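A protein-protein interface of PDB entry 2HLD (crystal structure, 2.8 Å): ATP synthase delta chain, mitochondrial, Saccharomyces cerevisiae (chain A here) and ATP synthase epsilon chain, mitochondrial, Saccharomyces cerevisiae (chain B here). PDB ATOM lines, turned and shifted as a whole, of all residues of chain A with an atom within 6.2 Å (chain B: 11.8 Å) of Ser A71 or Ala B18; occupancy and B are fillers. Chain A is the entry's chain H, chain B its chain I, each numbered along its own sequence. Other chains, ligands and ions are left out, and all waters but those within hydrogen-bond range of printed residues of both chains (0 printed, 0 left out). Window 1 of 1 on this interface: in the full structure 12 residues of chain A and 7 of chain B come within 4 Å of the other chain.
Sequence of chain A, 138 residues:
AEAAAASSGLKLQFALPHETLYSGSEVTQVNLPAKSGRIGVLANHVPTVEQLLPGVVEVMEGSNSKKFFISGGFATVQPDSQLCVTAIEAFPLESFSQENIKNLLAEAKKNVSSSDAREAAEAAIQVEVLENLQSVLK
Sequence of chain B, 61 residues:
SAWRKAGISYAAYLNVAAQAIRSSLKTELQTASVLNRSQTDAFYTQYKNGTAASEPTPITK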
ATOM      1  N   LEU A  52       8.031  27.722  -9.572  1.00  0.00           N
ATOM      2  CA  LEU A  52       6.744  27.338 -10.121  1.00  0.00           C
ATOM      3  C   LEU A  52       5.658  28.034  -9.317  1.00  0.00           C
ATOM      4  O   LEU A  52       5.616  27.910  -8.100  1.00  0.00           O
ATOM      5  CB  LEU A  52       6.562  25.819 -10.080  1.00  0.00           C
ATOM      6  CG  LEU A  52       7.476  24.897 -10.908  1.00  0.00           C
ATOM      7  CD1 LEU A  52       6.908  23.481 -10.953  1.00  0.00           C
ATOM      8  CD2 LEU A  52       7.726  25.404 -12.335  1.00  0.00           C
ATOM      9  N   LEU A  53       4.805  28.793 -10.005  1.00  0.00           N
ATOM     10  CA  LEU A  53       3.660  29.483  -9.389  1.00  0.00           C
ATOM     11  C   LEU A  53       2.505  28.484  -9.201  1.00  0.00           C
ATOM     12  O   LEU A  53       2.504  27.435  -9.849  1.00  0.00           O
ATOM     13  CB  LEU A  53       3.225  30.669 -10.270  1.00  0.00           C
ATOM     14  N   PRO A  54       1.549  28.782  -8.310  1.00  0.00           N
ATOM     15  CA  PRO A  54       0.374  27.910  -8.111  1.00  0.00           C
ATOM     16  C   PRO A  54      -0.554  27.781  -9.347  1.00  0.00           C
ATOM     17  O   PRO A  54      -1.620  28.418  -9.399  1.00  0.00           O
ATOM     18  CB  PRO A  54      -0.366  28.572  -6.931  1.00  0.00           C
ATOM     19  CG  PRO A  54       0.624  29.495  -6.294  1.00  0.00           C
ATOM     20  CD  PRO A  54       1.529  29.943  -7.398  1.00  0.00           C
ATOM     21  N   GLY A  55      -0.152  26.942 -10.309  1.00  0.00           N
ATOM     22  CA  GLY A  55      -0.869  26.762 -11.587  1.00  0.00           C
ATOM     23  C   GLY A  55      -0.888  25.333 -12.125  1.00  0.00           C
ATOM     24  O   GLY A  55      -0.612  24.375 -11.394  1.00  0.00           O
ATOM     25  N   PHE A  69      -3.244  20.191 -11.217  1.00  0.00           N
ATOM     26  CA  PHE A  69      -3.158  21.454 -10.493  1.00  0.00           C
ATOM     27  C   PHE A  69      -2.206  21.347  -9.289  1.00  0.00           C
ATOM     28  O   PHE A  69      -2.229  20.357  -8.537  1.00  0.00           O
ATOM     29  CB  PHE A  69      -4.515  22.036 -10.113  1.00  0.00           C
ATOM     30  CG  PHE A  69      -4.434  23.460  -9.636  1.00  0.00           C
ATOM     31  CD1 PHE A  69      -4.125  24.485 -10.524  1.00  0.00           C
ATOM     32  CD2 PHE A  69      -4.641  23.774  -8.293  1.00  0.00           C
ATOM     33  CE1 PHE A  69      -4.039  25.815 -10.083  1.00  0.00           C
ATOM     34  CE2 PHE A  69      -4.566  25.098  -7.837  1.00  0.00           C
ATOM     35  CZ  PHE A  69      -4.263  26.121  -8.733  1.00  0.00           C
ATOM     36  N   ILE A  70      -1.376  22.385  -9.135  1.00  0.00           N
ATOM     37  CA  ILE A  70      -0.161  22.343  -8.315  1.00  0.00           C
ATOM     38  C   ILE A  70       0.013  23.558  -7.383  1.00  0.00           C
ATOM     39  O   ILE A  70      -0.392  24.685  -7.715  1.00  0.00           O
ATOM     40  CB  ILE A  70       1.077  22.066  -9.243  1.00  0.00           C
ATOM     41  CG1 ILE A  70       1.485  20.599  -9.121  1.00  0.00           C
ATOM     42  CG2 ILE A  70       2.262  23.020  -8.977  1.00  0.00           C
ATOM     43  CD1 ILE A  70       2.281  20.075 -10.260  1.00  0.00           C
ATOM     44  N   SER A  71       0.596  23.290  -6.209  1.00  0.00           N
ATOM     45  CA  SER A  71       0.848  24.293  -5.155  1.00  0.00           C
ATOM     46  C   SER A  71       1.894  25.338  -5.548  1.00  0.00           C
ATOM     47  O   SER A  71       1.750  26.533  -5.261  1.00  0.00           O
ATOM     48  CB  SER A  71       1.321  23.595  -3.875  1.00  0.00           C
ATOM     49  OG  SER A  71       2.557  22.919  -4.085  1.00  0.00           O
ATOM     50  N   GLY A  72       2.949  24.862  -6.199  1.00  0.00           N
ATOM     51  CA  GLY A  72       4.106  25.676  -6.536  1.00  0.00           C
ATOM     52  C   GLY A  72       5.376  24.936  -6.156  1.00  0.00           C
ATOM     53  O   GLY A  72       5.329  23.782  -5.715  1.00  0.00           O
ATOM     54  N   GLY A  73       6.517  25.596  -6.316  1.00  0.00           N
ATOM     55  CA  GLY A  73       7.787  24.923  -6.134  1.00  0.00           C
ATOM     56  C   GLY A  73       8.807  25.383  -7.140  1.00  0.00           C
ATOM     57  O   GLY A  73       9.044  26.585  -7.259  1.00  0.00           O
ATOM     58  N   ALA A  87       6.780  20.094  -6.218  1.00  0.00           N
ATOM     59  CA  ALA A  87       5.698  20.895  -5.646  1.00  0.00           C
ATOM     60  C   ALA A  87       5.134  20.135  -4.455  1.00  0.00           C
ATOM     61  O   ALA A  87       5.359  18.934  -4.340  1.00  0.00           O
ATOM     62  CB  ALA A  87       4.612  21.149  -6.679  1.00  0.00           C
ATOM     63  N   ILE A  88       4.411  20.832  -3.577  1.00  0.00           N
ATOM     64  CA  ILE A  88       3.759  20.188  -2.428  1.00  0.00           C
ATOM     65  C   ILE A  88       2.515  19.379  -2.864  1.00  0.00           C
ATOM     66  O   ILE A  88       2.483  18.144  -2.752  1.00  0.00           O
ATOM     67  CB  ILE A  88       3.383  21.219  -1.324  1.00  0.00           C
ATOM     68  CG1 ILE A  88       4.515  22.224  -1.094  1.00  0.00           C
ATOM     69  CG2 ILE A  88       3.013  20.496  -0.026  1.00  0.00           C
ATOM     70  CD1 ILE A  88       4.043  23.524  -0.479  1.00  0.00           C
ATOM     71  N   GLU A  89       1.504  20.089  -3.365  1.00  0.00           N
ATOM     72  CA  GLU A  89       0.265  19.461  -3.799  1.00  0.00           C
ATOM     73  C   GLU A  89       0.224  19.332  -5.318  1.00  0.00           C
ATOM     74  O   GLU A  89       0.491  20.302  -6.035  1.00  0.00           O
ATOM     75  CB  GLU A  89      -0.961  20.229  -3.271  1.00  0.00           C
ATOM     76  CG  GLU A  89      -1.245  20.060  -1.772  1.00  0.00           C
ATOM     77  CD  GLU A  89      -1.163  18.608  -1.282  1.00  0.00           C
ATOM     78  OE1 GLU A  89      -1.641  17.688  -1.983  1.00  0.00           O
ATOM     79  OE2 GLU A  89      -0.609  18.375  -0.184  1.00  0.00           O
ATOM     80  N   ALA A  90      -0.089  18.124  -5.793  1.00  0.00           N
ATOM     81  CA  ALA A  90      -0.281  17.867  -7.227  1.00  0.00           C
ATOM     82  C   ALA A  90      -1.501  16.976  -7.498  1.00  0.00           C
ATOM     83  O   ALA A  90      -1.382  15.760  -7.703  1.00  0.00           O
ATOM     84  CB  ALA A  90       0.981  17.269  -7.839  1.00  0.00           C
ATOM     85  N   SER B   9       7.641  33.392   5.104  1.00  0.00           N
ATOM     86  CA  SER B   9       8.656  32.916   4.141  1.00  0.00           C
ATOM     87  C   SER B   9       8.088  32.272   2.869  1.00  0.00           C
ATOM     88  O   SER B   9       6.883  32.047   2.776  1.00  0.00           O
ATOM     89  CB  SER B   9       9.617  31.944   4.830  1.00  0.00           C
ATOM     90  OG  SER B   9       8.928  31.032   5.677  1.00  0.00           O
ATOM     91  N   TYR B  10       8.964  31.973   1.905  1.00  0.00           N
ATOM     92  CA  TYR B  10       8.558  31.356   0.623  1.00  0.00           C
ATOM     93  C   TYR B  10       7.947  29.955   0.757  1.00  0.00           C
ATOM     94  O   TYR B  10       7.098  29.576  -0.045  1.00  0.00           O
ATOM     95  CB  TYR B  10       9.715  31.344  -0.397  1.00  0.00           C
ATOM     96  CG  TYR B  10       9.410  30.640  -1.728  1.00  0.00           C
ATOM     97  CD1 TYR B  10       8.567  31.221  -2.686  1.00  0.00           C
ATOM     98  CD2 TYR B  10       9.977  29.396  -2.030  1.00  0.00           C
ATOM     99  CE1 TYR B  10       8.291  30.569  -3.906  1.00  0.00           C
ATOM    100  CE2 TYR B  10       9.707  28.743  -3.243  1.00  0.00           C
ATOM    101  CZ  TYR B  10       8.869  29.333  -4.176  1.00  0.00           C
ATOM    102  OH  TYR B  10       8.608  28.679  -5.369  1.00  0.00           O
ATOM    103  N   ALA B  11       8.375  29.187   1.757  1.00  0.00           N
ATOM    104  CA  ALA B  11       7.824  27.850   1.979  1.00  0.00           C
ATOM    105  C   ALA B  11       6.587  27.907   2.879  1.00  0.00           C
ATOM    106  O   ALA B  11       5.758  26.989   2.873  1.00  0.00           O
ATOM    107  CB  ALA B  11       8.878  26.937   2.567  1.00  0.00           C
ATOM    108  N   ALA B  12       6.485  28.982   3.662  1.00  0.00           N
ATOM    109  CA  ALA B  12       5.295  29.256   4.454  1.00  0.00           C
ATOM    110  C   ALA B  12       4.185  29.725   3.511  1.00  0.00           C
ATOM    111  O   ALA B  12       3.034  29.304   3.635  1.00  0.00           O
ATOM    112  CB  ALA B  12       5.592  30.304   5.516  1.00  0.00           C
ATOM    113  N   TYR B  13       4.554  30.591   2.565  1.00  0.00           N
ATOM    114  CA  TYR B  13       3.654  31.039   1.505  1.00  0.00           C
ATOM    115  C   TYR B  13       3.170  29.845   0.669  1.00  0.00           C
ATOM    116  O   TYR B  13       1.964  29.660   0.507  1.00  0.00           O
ATOM    117  CB  TYR B  13       4.310  32.162   0.658  1.00  0.00           C
ATOM    118  CG  TYR B  13       4.015  32.142  -0.836  1.00  0.00           C
ATOM    119  CD1 TYR B  13       4.768  31.338  -1.693  1.00  0.00           C
ATOM    120  CD2 TYR B  13       3.006  32.935  -1.395  1.00  0.00           C
ATOM    121  CE1 TYR B  13       4.522  31.293  -3.071  1.00  0.00           C
ATOM    122  CE2 TYR B  13       2.751  32.905  -2.788  1.00  0.00           C
ATOM    123  CZ  TYR B  13       3.520  32.072  -3.615  1.00  0.00           C
ATOM    124  OH  TYR B  13       3.318  31.997  -4.981  1.00  0.00           O
ATOM    125  N   LEU B  14       4.098  29.026   0.176  1.00  0.00           N
ATOM    126  CA  LEU B  14       3.743  27.802  -0.546  1.00  0.00           C
ATOM    127  C   LEU B  14       2.859  26.846   0.264  1.00  0.00           C
ATOM    128  O   LEU B  14       2.023  26.149  -0.310  1.00  0.00           O
ATOM    129  CB  LEU B  14       4.990  27.053  -1.011  1.00  0.00           C
ATOM    130  CG  LEU B  14       5.631  27.356  -2.364  1.00  0.00           C
ATOM    131  CD1 LEU B  14       6.512  26.169  -2.746  1.00  0.00           C
ATOM    132  CD2 LEU B  14       4.612  27.642  -3.470  1.00  0.00           C
ATOM    133  N   ASN B  15       3.063  26.816   1.583  1.00  0.00           N
ATOM    134  CA  ASN B  15       2.261  26.002   2.497  1.00  0.00           C
ATOM    135  C   ASN B  15       0.789  26.413   2.460  1.00  0.00           C
ATOM    136  O   ASN B  15      -0.103  25.573   2.274  1.00  0.00           O
ATOM    137  CB  ASN B  15       2.805  26.111   3.929  1.00  0.00           C
ATOM    138  CG  ASN B  15       1.846  25.541   4.982  1.00  0.00           C
ATOM    139  OD1 ASN B  15       1.327  26.274   5.831  1.00  0.00           O
ATOM    140  ND2 ASN B  15       1.611  24.234   4.929  1.00  0.00           N
ATOM    141  N   VAL B  16       0.557  27.713   2.635  1.00  0.00           N
ATOM    142  CA  VAL B  16      -0.783  28.289   2.611  1.00  0.00           C
ATOM    143  C   VAL B  16      -1.491  28.017   1.274  1.00  0.00           C
ATOM    144  O   VAL B  16      -2.684  27.703   1.253  1.00  0.00           O
ATOM    145  CB  VAL B  16      -0.737  29.805   2.985  1.00  0.00           C
ATOM    146  CG1 VAL B  16      -1.802  30.617   2.241  1.00  0.00           C
ATOM    147  CG2 VAL B  16      -0.860  29.983   4.513  1.00  0.00           C
ATOM    148  N   ALA B  17      -0.733  28.103   0.177  1.00  0.00           N
ATOM    149  CA  ALA B  17      -1.231  27.826  -1.178  1.00  0.00           C
ATOM    150  C   ALA B  17      -1.476  26.333  -1.418  1.00  0.00           C
ATOM    151  O   ALA B  17      -2.124  25.954  -2.392  1.00  0.00           O
ATOM    152  CB  ALA B  17      -0.262  28.383  -2.230  1.00  0.00           C
ATOM    153  N   ALA B  18      -0.939  25.495  -0.533  1.00  0.00           N
ATOM    154  CA  ALA B  18      -1.143  24.050  -0.588  1.00  0.00           C
ATOM    155  C   ALA B  18      -2.228  23.631   0.397  1.00  0.00           C
ATOM    156  O   ALA B  18      -2.786  22.533   0.275  1.00  0.00           O
ATOM    157  CB  ALA B  18       0.168  23.305  -0.301  1.00  0.00           C
ATOM    158  N   GLN B  19      -2.516  24.505   1.366  1.00  0.00           N
ATOM    159  CA  GLN B  19      -3.538  24.231   2.382  1.00  0.00           C
ATOM    160  C   GLN B  19      -4.898  24.780   1.990  1.00  0.00           C
ATOM    161  O   GLN B  19      -5.925  24.311   2.491  1.00  0.00           O
ATOM    162  CB  GLN B  19      -3.156  24.776   3.763  1.00  0.00           C
ATOM    163  CG  GLN B  19      -3.775  23.960   4.911  1.00  0.00           C
ATOM    164  CD  GLN B  19      -4.272  24.810   6.073  1.00  0.00           C
ATOM    165  OE1 GLN B  19      -3.974  26.003   6.158  1.00  0.00           O
ATOM    166  NE2 GLN B  19      -5.036  24.194   6.971  1.00  0.00           N
ATOM    167  N   ALA B  20      -4.897  25.793   1.122  1.00  0.00           N
ATOM    168  CA  ALA B  20      -6.128  26.268   0.501  1.00  0.00           C
ATOM    169  C   ALA B  20      -6.571  25.206  -0.502  1.00  0.00           C
ATOM    170  O   ALA B  20      -7.629  24.602  -0.324  1.00  0.00           O
ATOM    171  CB  ALA B  20      -5.929  27.625  -0.163  1.00  0.00           C
ATOM    172  N   ILE B  21      -5.745  24.944  -1.514  1.00  0.00           N
ATOM    173  CA  ILE B  21      -5.980  23.830  -2.450  1.00  0.00           C
ATOM    174  C   ILE B  21      -6.191  22.462  -1.748  1.00  0.00           C
ATOM    175  O   ILE B  21      -6.399  21.433  -2.395  1.00  0.00           O
ATOM    176  CB  ILE B  21      -4.851  23.753  -3.515  1.00  0.00           C
ATOM    177  N   ARG B  22      -6.128  22.461  -0.422  1.00  0.00           N
ATOM    178  CA  ARG B  22      -6.601  21.328   0.350  1.00  0.00           C
ATOM    179  C   ARG B  22      -8.063  21.616   0.688  1.00  0.00           C
ATOM    180  O   ARG B  22      -8.960  21.142  -0.015  1.00  0.00           O
ATOM    181  CB  ARG B  22      -5.747  21.107   1.603  1.00  0.00           C
ATOM    182  N   SER B  23      -8.292  22.429   1.725  1.00  0.00           N
ATOM    183  CA  SER B  23      -9.644  22.816   2.155  1.00  0.00           C
ATOM    184  C   SER B  23     -10.500  23.416   1.017  1.00  0.00           C
ATOM    185  O   SER B  23     -11.305  22.722   0.375  1.00  0.00           O
ATOM    186  CB  SER B  23      -9.567  23.787   3.340  1.00  0.00           C
ATOM    187  N   LEU B  29     -12.526  12.906  -1.886  1.00  0.00           N
ATOM    188  CA  LEU B  29     -11.131  12.891  -2.323  1.00  0.00           C
ATOM    189  C   LEU B  29     -10.233  13.411  -1.195  1.00  0.00           C
ATOM    190  O   LEU B  29      -9.003  13.301  -1.267  1.00  0.00           O
ATOM    191  CB  LEU B  29     -10.950  13.742  -3.586  1.00  0.00           C
ATOM    192  CG  LEU B  29     -11.543  13.205  -4.900  1.00  0.00           C
ATOM    193  CD1 LEU B  29     -11.752  14.338  -5.913  1.00  0.00           C
ATOM    194  CD2 LEU B  29     -10.706  12.063  -5.510  1.00  0.00           C
ATOM    195  N   GLN B  30     -10.869  13.961  -0.157  1.00  0.00           N
ATOM    196  CA  GLN B  30     -10.189  14.517   1.005  1.00  0.00           C
ATOM    197  C   GLN B  30     -10.045  13.499   2.131  1.00  0.00           C
ATOM    198  O   GLN B  30     -10.579  13.701   3.227  1.00  0.00           O
ATOM    199  CB  GLN B  30     -10.942  15.747   1.509  1.00  0.00           C
ATOM    200  CG  GLN B  30     -10.736  17.003   0.664  1.00  0.00           C
ATOM    201  CD  GLN B  30     -11.234  18.277   1.349  1.00  0.00           C
ATOM    202  OE1 GLN B  30     -11.763  18.236   2.477  1.00  0.00           O
ATOM    203  NE2 GLN B  30     -11.067  19.412   0.667  1.00  0.00           N
ATOM    204  N   SER B  33      -5.305  11.168   5.610  1.00  0.00           N
ATOM    205  CA  SER B  33      -3.924  11.655   5.494  1.00  0.00           C
ATOM    206  C   SER B  33      -3.804  13.009   4.766  1.00  0.00           C
ATOM    207  O   SER B  33      -2.698  13.556   4.645  1.00  0.00           O
ATOM    208  CB  SER B  33      -3.046  10.602   4.810  1.00  0.00           C
ATOM    209  OG  SER B  33      -3.555  10.286   3.529  1.00  0.00           O
ATOM    210  N   VAL B  34      -4.938  13.519   4.274  1.00  0.00           N
ATOM    211  CA  VAL B  34      -5.044  14.874   3.723  1.00  0.00           C
ATOM    212  C   VAL B  34      -5.433  15.833   4.848  1.00  0.00           C
ATOM    213  O   VAL B  34      -4.775  16.846   5.066  1.00  0.00           O
ATOM    214  CB  VAL B  34      -6.052  14.950   2.517  1.00  0.00           C
ATOM    215  CG1 VAL B  34      -6.501  16.390   2.224  1.00  0.00           C
ATOM    216  CG2 VAL B  34      -5.457  14.299   1.260  1.00  0.00           C
ATOM    217  N   LEU B  35      -6.492  15.502   5.578  1.00  0.00           N
ATOM    218  CA  LEU B  35      -6.898  16.313   6.722  1.00  0.00           C
ATOM    219  C   LEU B  35      -5.788  16.377   7.785  1.00  0.00           C
ATOM    220  O   LEU B  35      -5.732  17.332   8.563  1.00  0.00           O
ATOM    221  CB  LEU B  35      -8.213  15.792   7.321  1.00  0.00           C
ATOM    222  N   ASN B  36      -4.912  15.367   7.790  1.00  0.00           N
ATOM    223  CA  ASN B  36      -3.801  15.254   8.756  1.00  0.00           C
ATOM    224  C   ASN B  36      -2.568  16.074   8.358  1.00  0.00           C
ATOM    225  O   ASN B  36      -1.952  16.735   9.191  1.00  0.00           O
ATOM    226  CB  ASN B  36      -3.419  13.776   8.983  1.00  0.00           C
ATOM    227  CG  ASN B  36      -4.263  13.090  10.088  1.00  0.00           C
ATOM    228  OD1 ASN B  36      -5.207  13.668  10.648  1.00  0.00           O
ATOM    229  ND2 ASN B  36      -3.908  11.848  10.400  1.00  0.00           N
ATOM    230  N   ARG B  37      -2.231  16.008   7.073  1.00  0.00           N
ATOM    231  CA  ARG B  37      -1.202  16.825   6.446  1.00  0.00           C
ATOM    232  C   ARG B  37      -1.494  18.323   6.614  1.00  0.00           C
ATOM    233  O   ARG B  37      -0.625  19.169   6.366  1.00  0.00           O
ATOM    234  CB  ARG B  37      -1.097  16.425   4.971  1.00  0.00           C
ATOM    235  CG  ARG B  37      -0.747  17.529   3.986  1.00  0.00           C
ATOM    236  CD  ARG B  37      -0.956  17.150   2.531  1.00  0.00           C
ATOM    237  NE  ARG B  37      -0.583  15.759   2.269  1.00  0.00           N
ATOM    238  CZ  ARG B  37      -1.019  15.033   1.240  1.00  0.00           C
ATOM    239  NH1 ARG B  37      -1.846  15.549   0.337  1.00  0.00           N
ATOM    240  NH2 ARG B  37      -0.623  13.775   1.114  1.00  0.00           N
ATOM    241  N   SER B  38      -2.710  18.643   7.058  1.00  0.00           N
ATOM    242  CA  SER B  38      -3.090  20.025   7.346  1.00  0.00           C
ATOM    243  C   SER B  38      -3.172  20.289   8.864  1.00  0.00           C
ATOM    244  O   SER B  38      -3.669  21.335   9.284  1.00  0.00           O
ATOM    245  CB  SER B  38      -4.414  20.395   6.638  1.00  0.00           C
ATOM    246  OG  SER B  38      -4.246  20.722   5.253  1.00  0.00           O
ATOM    247  N   GLN B  39      -2.674  19.353   9.679  1.00  0.00           N
ATOM    248  CA  GLN B  39      -2.760  19.460  11.156  1.00  0.00           C
ATOM    249  C   GLN B  39      -1.434  19.202  11.906  1.00  0.00           C
ATOM    250  O   GLN B  39      -0.775  18.177  11.695  1.00  0.00           O
ATOM    251  CB  GLN B  39      -3.865  18.535  11.704  1.00  0.00           C
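Of the 24 printed residues of chain B, 5 touch a printed residue of chain A. Hydrophobic or aromatic side chains of chain B that line the printed part of chain A: Tyr B10, Tyr B13, Leu B14 and Ala B18. Of the 13 printed residues of chain A, 6 touch a printed residue of chain B. Hydrophobic or aromatic side chains of chain A that line the printed part of chain B: Pro A54 and Ile A88.
OH of Tyr B10 sits at hydrogen-bond distance from O of Gly A73, at 2.9 Å. The side-chain carboxylate (OE2) of Glu A89 lies within salt-bridge range of the guanidinium group (NH1) of Arg B37.
Among the printed residues, pairs that only touch across the chains: Ile A88 with Leu B14, Ser A71 with Leu B14, Glu A89 with Ala B18, Gly A73 with Leu B14, Pro A54 with Tyr B13, Gly A72 with Leu B14, Ser A71 with Ala B18 and Ile A88 with Ala B18.
Leu A53 touches none of the printed residues of chain B. No residue of chain B comes within 4 Å of Gly A55. No residue of chain B comes within 4 Å of Ile A70. Of chain B, only Leu B14 (3.6 Å) and Ala B18 (3.8 Å) come within 4 Å of Ser A71. Of chain B, only Leu B14 (3.7 Å) comes within 4 Å of Gly A72. Ala A87 touches none of the printed residues of chain B. Of the printed residues of chain A, Leu B14 touches Ser A71 (3.6 Å), Gly A72 (3.7 Å), Gly A73 (3.6 Å) and Ile A88 (3.3 Å). Ala B18 touches just these residues of chain A: Ser A71 (3.8 Å), Ile A88 (3.9 Å) and Glu A89 (3.6 Å). Of the printed residues of chain A, Arg B37 touches Glu A89.
N of Leu A52 sits at hydrogen-bond distance from O of Gly A73, at 2.8 Å. The backbone NH (N) of Ile A88 lies within hydrogen-bond range of the side-chain hydroxyl (OG) of Ser A71. The backbone NH of Ser A71 sits at hydrogen-bond distance from the backbone carbonyl oxygen of Glu A89 (3.0 Å).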
